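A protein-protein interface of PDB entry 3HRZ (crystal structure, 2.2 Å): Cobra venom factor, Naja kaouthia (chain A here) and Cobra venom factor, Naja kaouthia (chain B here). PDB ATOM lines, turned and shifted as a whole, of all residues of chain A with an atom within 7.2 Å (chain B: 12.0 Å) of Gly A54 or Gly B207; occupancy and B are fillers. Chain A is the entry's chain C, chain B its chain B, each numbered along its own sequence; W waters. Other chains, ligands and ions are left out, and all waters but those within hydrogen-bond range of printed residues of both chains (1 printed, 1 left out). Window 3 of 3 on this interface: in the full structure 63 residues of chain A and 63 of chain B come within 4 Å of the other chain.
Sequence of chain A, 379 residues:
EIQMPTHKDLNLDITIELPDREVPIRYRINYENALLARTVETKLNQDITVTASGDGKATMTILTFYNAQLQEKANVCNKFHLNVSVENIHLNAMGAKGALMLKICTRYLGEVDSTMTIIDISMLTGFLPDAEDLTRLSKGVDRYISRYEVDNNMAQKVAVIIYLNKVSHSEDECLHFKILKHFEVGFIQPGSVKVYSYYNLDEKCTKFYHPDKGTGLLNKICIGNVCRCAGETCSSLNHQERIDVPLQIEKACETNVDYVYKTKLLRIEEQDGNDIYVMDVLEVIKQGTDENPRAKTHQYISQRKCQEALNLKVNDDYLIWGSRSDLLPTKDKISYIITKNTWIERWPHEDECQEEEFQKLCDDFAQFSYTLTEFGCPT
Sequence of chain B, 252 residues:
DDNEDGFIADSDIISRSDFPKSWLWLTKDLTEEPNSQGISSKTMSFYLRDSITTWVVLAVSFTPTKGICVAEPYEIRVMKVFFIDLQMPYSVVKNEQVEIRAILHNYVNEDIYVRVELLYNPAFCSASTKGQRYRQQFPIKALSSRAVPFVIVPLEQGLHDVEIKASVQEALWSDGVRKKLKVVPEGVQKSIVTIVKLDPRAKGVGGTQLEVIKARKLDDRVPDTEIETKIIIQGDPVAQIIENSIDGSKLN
No residue of chain B comes within 4 Å of Asp A13.
Of chain B, only Gly B207 and Thr B208 come within 4 Å of Ser A53.
Gly A54 touches two residues of chain B.
No residue of chain B comes within 4 Å of Asp A55.
Of chain B, only Pro B200 (3.6 Å) comes within 4 Å of Gly A56.
Of the printed residues of chain B, Lys A57 touches Leu B198, Asp B199, Gly B235 and Asp B236.
Of the printed residues of chain A, Leu B198 touches Lys A57.
Of the printed residues of chain A, Asp B199 touches Lys A57.
Arg B201 touches none of the printed residues of chain A.
No residue of chain A comes within 4 Å of Gly B206.
Gly B207 touches three residues of chain A.
Of the printed residues of chain A, Gln B209 touches Ala A52 (2.8 Å).
The nearest residue of chain B that does not touch Gly A54 is Arg B201 (4.3 Å).
The nearest printed residue of chain A that does not touch Pro B200 is Ser A53 (4.1 Å).
Among the printed residues, pairs that only touch across the chains: Leu A10 with Asp B236, Leu A12 with Pro B200, Ala A52 with Pro B200, Ala A52 with Gly B207, Ala A52 with Thr B208, Ser A53 with Gly B207, Gly A54 with Pro B200, Gly A56 with Pro B200, Lys A57 with Leu B198, Lys A57 with Asp B199 and Lys A57 with Gly B235.
Hydrophobic or aromatic side chains of chain B that line the printed part of chain A: Pro B200.
Printed residues of chain A that touch a printed residue of chain B: Leu A10, Leu A12, Ala A52, Ser A53, Gly A54, Gly A56 and Lys A57.
Among the printed residues, 15 pairs touch across the chains.
Water W1 bridges the side-chain carboxylate of Asp B199 (2.5 Å) and the side-chain amino group of Lys A57 (3.2 Å).
N of Asp B236 sits at hydrogen-bond distance from O of Lys A57 (3.0 Å).
The backbone carbonyl oxygen (O) of Gly B207 lies within hydrogen-bond range of the backbone NH (N) of Gly A54 (3.3 Å).
The backbone NH of Gln B209 is in hydrogen-bond range of the backbone carbonyl oxygen of Ala A52 (2.8 Å).
The side-chain hydroxyl (OG) of Ser A53 sits at hydrogen-bond distance from the side-chain hydroxyl (OG1) of Thr B208, at 3.1 Å.
O of Lys B197 is in hydrogen-bond range of NE2 of Gln B209, at 3.1 Å.
OE1 of Gln B209 is in hydrogen-bond range of N of Asp B199, at 2.8 Å.
N of Asp A13 lies within hydrogen-bond range of O of Ser A53, at 2.8 Å.
The side-chain carboxylate (OE2) of Glu B211 lies within hydrogen-bond range of the side-chain amide nitrogen (NE2) of Gln B209, at 3.1 Å.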
ATOM      1  N   ASP A   9     -34.859 -14.912  10.537  1.00  0.00           N
ATOM      2  CA  ASP A   9     -35.926 -15.909  10.608  1.00  0.00           C
ATOM      3  C   ASP A   9     -35.598 -17.079   9.683  1.00  0.00           C
ATOM      4  O   ASP A   9     -34.894 -18.022  10.062  1.00  0.00           O
ATOM      5  CB  ASP A   9     -37.257 -15.276  10.195  1.00  0.00           C
ATOM      6  CG  ASP A   9     -37.438 -13.878  10.757  1.00  0.00           C
ATOM      7  OD1 ASP A   9     -38.056 -13.039  10.067  1.00  0.00           O
ATOM      8  OD2 ASP A   9     -36.956 -13.620  11.883  1.00  0.00           O
ATOM      9  N   LEU A  10     -36.149 -17.020   8.477  1.00  0.00           N
ATOM     10  CA  LEU A  10     -35.631 -17.796   7.366  1.00  0.00           C
ATOM     11  C   LEU A  10     -34.916 -16.796   6.473  1.00  0.00           C
ATOM     12  O   LEU A  10     -35.522 -15.840   5.995  1.00  0.00           O
ATOM     13  CB  LEU A  10     -36.754 -18.515   6.607  1.00  0.00           C
ATOM     14  CG  LEU A  10     -36.515 -18.946   5.149  1.00  0.00           C
ATOM     15  CD1 LEU A  10     -35.157 -19.612   4.936  1.00  0.00           C
ATOM     16  CD2 LEU A  10     -37.635 -19.857   4.667  1.00  0.00           C
ATOM     17  N   ASN A  11     -33.619 -17.008   6.275  1.00  0.00           N
ATOM     18  CA  ASN A  11     -32.815 -16.129   5.451  1.00  0.00           C
ATOM     19  C   ASN A  11     -31.674 -16.930   4.867  1.00  0.00           C
ATOM     20  O   ASN A  11     -30.631 -17.079   5.500  1.00  0.00           O
ATOM     21  CB  ASN A  11     -32.266 -14.980   6.285  1.00  0.00           C
ATOM     22  CG  ASN A  11     -32.199 -13.671   5.513  1.00  0.00           C
ATOM     23  OD1 ASN A  11     -32.912 -13.473   4.526  1.00  0.00           O
ATOM     24  ND2 ASN A  11     -31.347 -12.760   5.974  1.00  0.00           N
ATOM     25  N   LEU A  12     -31.885 -17.455   3.662  1.00  0.00           N
ATOM     26  CA  LEU A  12     -30.927 -18.341   3.014  1.00  0.00           C
ATOM     27  C   LEU A  12     -30.361 -17.729   1.759  1.00  0.00           C
ATOM     28  O   LEU A  12     -31.105 -17.274   0.892  1.00  0.00           O
ATOM     29  CB  LEU A  12     -31.605 -19.631   2.595  1.00  0.00           C
ATOM     30  CG  LEU A  12     -31.563 -20.848   3.502  1.00  0.00           C
ATOM     31  CD1 LEU A  12     -31.774 -22.070   2.621  1.00  0.00           C
ATOM     32  CD2 LEU A  12     -30.224 -20.920   4.225  1.00  0.00           C
ATOM     33  N   ASP A  13     -29.044 -17.735   1.646  1.00  0.00           N
ATOM     34  CA  ASP A  13     -28.416 -17.373   0.387  1.00  0.00           C
ATOM     35  C   ASP A  13     -27.969 -18.639  -0.313  1.00  0.00           C
ATOM     36  O   ASP A  13     -27.196 -19.420   0.246  1.00  0.00           O
ATOM     37  CB  ASP A  13     -27.241 -16.428   0.618  1.00  0.00           C
ATOM     38  CG  ASP A  13     -27.695 -15.040   1.007  1.00  0.00           C
ATOM     39  OD1 ASP A  13     -28.072 -14.266   0.098  1.00  0.00           O
ATOM     40  OD2 ASP A  13     -27.682 -14.729   2.220  1.00  0.00           O
ATOM     41  N   ALA A  52     -24.967 -22.813   0.417  1.00  0.00           N
ATOM     42  CA  ALA A  52     -26.022 -22.191   1.203  1.00  0.00           C
ATOM     43  C   ALA A  52     -25.449 -21.562   2.464  1.00  0.00           C
ATOM     44  O   ALA A  52     -24.700 -22.207   3.214  1.00  0.00           O
ATOM     45  CB  ALA A  52     -27.099 -23.195   1.538  1.00  0.00           C
ATOM     46  N   SER A  53     -25.795 -20.296   2.684  1.00  0.00           N
ATOM     47  CA  SER A  53     -25.378 -19.569   3.877  1.00  0.00           C
ATOM     48  C   SER A  53     -26.598 -18.988   4.571  1.00  0.00           C
ATOM     49  O   SER A  53     -27.534 -18.553   3.912  1.00  0.00           O
ATOM     50  CB  SER A  53     -24.442 -18.414   3.497  1.00  0.00           C
ATOM     51  OG  SER A  53     -23.392 -18.860   2.659  1.00  0.00           O
ATOM     52  N   GLY A  54     -26.583 -18.962   5.899  1.00  0.00           N
ATOM     53  CA  GLY A  54     -27.604 -18.233   6.630  1.00  0.00           C
ATOM     54  C   GLY A  54     -28.386 -19.040   7.644  1.00  0.00           C
ATOM     55  O   GLY A  54     -27.875 -19.998   8.221  1.00  0.00           O
ATOM     56  N   ASP A  55     -29.644 -18.655   7.826  1.00  0.00           N
ATOM     57  CA  ASP A  55     -30.464 -19.128   8.935  1.00  0.00           C
ATOM     58  C   ASP A  55     -31.388 -20.286   8.587  1.00  0.00           C
ATOM     59  O   ASP A  55     -31.486 -21.264   9.331  1.00  0.00           O
ATOM     60  CB  ASP A  55     -31.323 -17.975   9.472  1.00  0.00           C
ATOM     61  CG  ASP A  55     -30.512 -16.935  10.209  1.00  0.00           C
ATOM     62  OD1 ASP A  55     -29.487 -17.308  10.819  1.00  0.00           O
ATOM     63  OD2 ASP A  55     -30.908 -15.747  10.185  1.00  0.00           O
ATOM     64  N   GLY A  56     -32.101 -20.160   7.478  1.00  0.00           N
ATOM     65  CA  GLY A  56     -33.154 -21.113   7.188  1.00  0.00           C
ATOM     66  C   GLY A  56     -32.732 -22.514   6.762  1.00  0.00           C
ATOM     67  O   GLY A  56     -31.554 -22.887   6.847  1.00  0.00           O
ATOM     68  N   LYS A  57     -33.729 -23.282   6.329  1.00  0.00           N
ATOM     69  CA  LYS A  57     -33.546 -24.606   5.765  1.00  0.00           C
ATOM     70  C   LYS A  57     -34.284 -24.669   4.445  1.00  0.00           C
ATOM     71  O   LYS A  57     -35.296 -23.996   4.250  1.00  0.00           O
ATOM     72  CB  LYS A  57     -34.129 -25.674   6.680  1.00  0.00           C
ATOM     73  CG  LYS A  57     -33.486 -25.759   8.032  1.00  0.00           C
ATOM     74  CD  LYS A  57     -33.660 -27.155   8.623  1.00  0.00           C
ATOM     75  CE  LYS A  57     -35.077 -27.394   9.114  1.00  0.00           C
ATOM     76  NZ  LYS A  57     -35.154 -28.561  10.049  1.00  0.00           N
ATOM     77  N   LYS B 197     -30.564 -31.887   1.589  1.00  0.00           N
ATOM     78  CA  LYS B 197     -31.110 -30.958   2.575  1.00  0.00           C
ATOM     79  C   LYS B 197     -30.142 -29.808   2.826  1.00  0.00           C
ATOM     80  O   LYS B 197     -29.024 -30.025   3.271  1.00  0.00           O
ATOM     81  CB  LYS B 197     -31.406 -31.684   3.885  1.00  0.00           C
ATOM     82  CG  LYS B 197     -32.494 -32.744   3.769  1.00  0.00           C
ATOM     83  CD  LYS B 197     -33.877 -32.111   3.792  1.00  0.00           C
ATOM     84  CE  LYS B 197     -34.966 -33.165   3.794  1.00  0.00           C
ATOM     85  NZ  LYS B 197     -36.315 -32.543   3.804  1.00  0.00           N
ATOM     86  N   LEU B 198     -30.569 -28.590   2.516  1.00  0.00           N
ATOM     87  CA  LEU B 198     -29.777 -27.409   2.828  1.00  0.00           C
ATOM     88  C   LEU B 198     -30.152 -26.892   4.210  1.00  0.00           C
ATOM     89  O   LEU B 198     -31.308 -26.566   4.486  1.00  0.00           O
ATOM     90  CB  LEU B 198     -29.981 -26.322   1.779  1.00  0.00           C
ATOM     91  CG  LEU B 198     -29.727 -26.783   0.344  1.00  0.00           C
ATOM     92  CD1 LEU B 198     -30.258 -25.759  -0.627  1.00  0.00           C
ATOM     93  CD2 LEU B 198     -28.239 -27.037   0.105  1.00  0.00           C
ATOM     94  N   ASP B 199     -29.157 -26.842   5.082  1.00  0.00           N
ATOM     95  CA  ASP B 199     -29.355 -26.456   6.465  1.00  0.00           C
ATOM     96  C   ASP B 199     -27.995 -26.086   7.054  1.00  0.00           C
ATOM     97  O   ASP B 199     -27.394 -26.864   7.797  1.00  0.00           O
ATOM     98  CB  ASP B 199     -29.987 -27.616   7.230  1.00  0.00           C
ATOM     99  CG  ASP B 199     -30.220 -27.298   8.695  1.00  0.00           C
ATOM    100  OD1 ASP B 199     -29.998 -26.136   9.117  1.00  0.00           O
ATOM    101  OD2 ASP B 199     -30.618 -28.221   9.432  1.00  0.00           O
ATOM    102  N   PRO B 200     -27.502 -24.891   6.703  1.00  0.00           N
ATOM    103  CA  PRO B 200     -26.150 -24.415   7.034  1.00  0.00           C
ATOM    104  C   PRO B 200     -25.873 -24.399   8.537  1.00  0.00           C
ATOM    105  O   PRO B 200     -24.744 -24.652   8.969  1.00  0.00           O
ATOM    106  CB  PRO B 200     -26.130 -22.987   6.479  1.00  0.00           C
ATOM    107  CG  PRO B 200     -27.202 -22.954   5.441  1.00  0.00           C
ATOM    108  CD  PRO B 200     -28.257 -23.937   5.874  1.00  0.00           C
ATOM    109  N   ARG B 201     -26.894 -24.086   9.327  1.00  0.00           N
ATOM    110  CA  ARG B 201     -26.754 -24.066  10.780  1.00  0.00           C
ATOM    111  C   ARG B 201     -26.344 -25.435  11.334  1.00  0.00           C
ATOM    112  O   ARG B 201     -25.525 -25.518  12.248  1.00  0.00           O
ATOM    113  CB  ARG B 201     -28.060 -23.593  11.430  1.00  0.00           C
ATOM    114  CG  ARG B 201     -28.085 -23.659  12.945  1.00  0.00           C
ATOM    115  CD  ARG B 201     -27.189 -22.607  13.582  1.00  0.00           C
ATOM    116  NE  ARG B 201     -27.398 -22.524  15.031  1.00  0.00           N
ATOM    117  CZ  ARG B 201     -26.691 -23.205  15.930  1.00  0.00           C
ATOM    118  NH1 ARG B 201     -25.717 -24.021  15.539  1.00  0.00           N
ATOM    119  NH2 ARG B 201     -26.958 -23.074  17.222  1.00  0.00           N
ATOM    120  N   ALA B 202     -26.912 -26.502  10.773  1.00  0.00           N
ATOM    121  CA  ALA B 202     -26.656 -27.861  11.255  1.00  0.00           C
ATOM    122  C   ALA B 202     -25.612 -28.628  10.447  1.00  0.00           C
ATOM    123  O   ALA B 202     -25.040 -29.602  10.944  1.00  0.00           O
ATOM    124  CB  ALA B 202     -27.958 -28.670  11.301  1.00  0.00           C
ATOM    125  N   LYS B 203     -25.374 -28.197   9.212  1.00  0.00           N
ATOM    126  CA  LYS B 203     -24.556 -28.962   8.265  1.00  0.00           C
ATOM    127  C   LYS B 203     -23.340 -28.204   7.714  1.00  0.00           C
ATOM    128  O   LYS B 203     -22.453 -28.804   7.096  1.00  0.00           O
ATOM    129  CB  LYS B 203     -25.427 -29.474   7.104  1.00  0.00           C
ATOM    130  CG  LYS B 203     -26.543 -30.399   7.554  1.00  0.00           C
ATOM    131  CD  LYS B 203     -27.423 -30.841   6.404  1.00  0.00           C
ATOM    132  CE  LYS B 203     -26.814 -32.039   5.672  1.00  0.00           C
ATOM    133  NZ  LYS B 203     -27.735 -32.562   4.624  1.00  0.00           N
ATOM    134  N   GLY B 204     -23.299 -26.896   7.945  1.00  0.00           N
ATOM    135  CA  GLY B 204     -22.257 -26.057   7.383  1.00  0.00           C
ATOM    136  C   GLY B 204     -21.038 -25.888   8.266  1.00  0.00           C
ATOM    137  O   GLY B 204     -20.899 -26.554   9.289  1.00  0.00           O
ATOM    138  N   VAL B 205     -20.150 -24.987   7.860  1.00  0.00           N
ATOM    139  CA  VAL B 205     -18.931 -24.705   8.602  1.00  0.00           C
ATOM    140  C   VAL B 205     -19.146 -23.490   9.485  1.00  0.00           C
ATOM    141  O   VAL B 205     -19.493 -23.605  10.662  1.00  0.00           O
ATOM    142  CB  VAL B 205     -17.762 -24.395   7.654  1.00  0.00           C
ATOM    143  CG1 VAL B 205     -16.446 -24.334   8.425  1.00  0.00           C
ATOM    144  CG2 VAL B 205     -17.690 -25.427   6.535  1.00  0.00           C
ATOM    145  N   GLY B 206     -18.925 -22.315   8.914  1.00  0.00           N
ATOM    146  CA  GLY B 206     -19.203 -21.082   9.619  1.00  0.00           C
ATOM    147  C   GLY B 206     -20.508 -20.566   9.072  1.00  0.00           C
ATOM    148  O   GLY B 206     -20.551 -19.506   8.448  1.00  0.00           O
ATOM    149  N   GLY B 207     -21.569 -21.344   9.277  1.00  0.00           N
ATOM    150  CA  GLY B 207     -22.875 -21.009   8.743  1.00  0.00           C
ATOM    151  C   GLY B 207     -22.941 -21.135   7.232  1.00  0.00           C
ATOM    152  O   GLY B 207     -23.865 -20.623   6.593  1.00  0.00           O
ATOM    153  N   THR B 208     -21.953 -21.819   6.661  1.00  0.00           N
ATOM    154  CA  THR B 208     -21.893 -22.037   5.222  1.00  0.00           C
ATOM    155  C   THR B 208     -21.823 -23.524   4.877  1.00  0.00           C
ATOM    156  O   THR B 208     -20.983 -24.254   5.388  1.00  0.00           O
ATOM    157  CB  THR B 208     -20.675 -21.330   4.608  1.00  0.00           C
ATOM    158  OG1 THR B 208     -21.012 -19.967   4.317  1.00  0.00           O
ATOM    159  CG2 THR B 208     -20.253 -22.027   3.323  1.00  0.00           C
ATOM    160  N   GLN B 209     -22.713 -23.967   4.003  1.00  0.00           N
ATOM    161  CA  GLN B 209     -22.755 -25.362   3.614  1.00  0.00           C
ATOM    162  C   GLN B 209     -22.420 -25.491   2.134  1.00  0.00           C
ATOM    163  O   GLN B 209     -22.989 -24.793   1.292  1.00  0.00           O
ATOM    164  CB  GLN B 209     -24.133 -25.953   3.895  1.00  0.00           C
ATOM    165  CG  GLN B 209     -24.305 -27.412   3.466  1.00  0.00           C
ATOM    166  CD  GLN B 209     -25.720 -27.907   3.708  1.00  0.00           C
ATOM    167  OE1 GLN B 209     -26.497 -27.252   4.400  1.00  0.00           O
ATOM    168  NE2 GLN B 209     -26.062 -29.058   3.141  1.00  0.00           N
ATOM    169  N   LEU B 210     -21.485 -26.380   1.825  1.00  0.00           N
ATOM    170  CA  LEU B 210     -21.045 -26.587   0.453  1.00  0.00           C
ATOM    171  C   LEU B 210     -21.333 -28.019   0.038  1.00  0.00           C
ATOM    172  O   LEU B 210     -20.872 -28.965   0.676  1.00  0.00           O
ATOM    173  CB  LEU B 210     -19.553 -26.267   0.314  1.00  0.00           C
ATOM    174  CG  LEU B 210     -18.931 -26.350  -1.086  1.00  0.00           C
ATOM    175  CD1 LEU B 210     -19.810 -25.653  -2.108  1.00  0.00           C
ATOM    176  CD2 LEU B 210     -17.523 -25.763  -1.113  1.00  0.00           C
ATOM    177  N   GLU B 211     -22.123 -28.168  -1.019  1.00  0.00           N
ATOM    178  CA  GLU B 211     -22.481 -29.478  -1.551  1.00  0.00           C
ATOM    179  C   GLU B 211     -22.023 -29.583  -2.999  1.00  0.00           C
ATOM    180  O   GLU B 211     -22.252 -28.671  -3.795  1.00  0.00           O
ATOM    181  CB  GLU B 211     -24.000 -29.686  -1.504  1.00  0.00           C
ATOM    182  CG  GLU B 211     -24.598 -29.745  -0.109  1.00  0.00           C
ATOM    183  CD  GLU B 211     -24.156 -30.974   0.664  1.00  0.00           C
ATOM    184  OE1 GLU B 211     -24.050 -32.059   0.045  1.00  0.00           O
ATOM    185  OE2 GLU B 211     -23.917 -30.849   1.889  1.00  0.00           O
ATOM    186  N   GLY B 235     -37.764 -23.746  -0.059  1.00  0.00           N
ATOM    187  CA  GLY B 235     -37.562 -23.361   1.319  1.00  0.00           C
ATOM    188  C   GLY B 235     -38.529 -24.133   2.195  1.00  0.00           C
ATOM    189  O   GLY B 235     -39.623 -24.476   1.753  1.00  0.00           O
ATOM    190  N   ASP B 236     -38.110 -24.438   3.417  1.00  0.00           N
ATOM    191  CA  ASP B 236     -39.004 -25.060   4.382  1.00  0.00           C
ATOM    192  C   ASP B 236     -39.666 -23.971   5.205  1.00  0.00           C
ATOM    193  O   ASP B 236     -38.994 -23.064   5.691  1.00  0.00           O
ATOM    194  CB  ASP B 236     -38.244 -26.017   5.301  1.00  0.00           C
ATOM    195  CG  ASP B 236     -37.882 -27.319   4.620  1.00  0.00           C
ATOM    196  OD1 ASP B 236     -38.137 -27.455   3.403  1.00  0.00           O
ATOM    197  OD2 ASP B 236     -37.337 -28.208   5.309  1.00  0.00           O
HETATM  198  O   HOH W   1     -32.228 -29.038  11.176  1.00  0.00           O
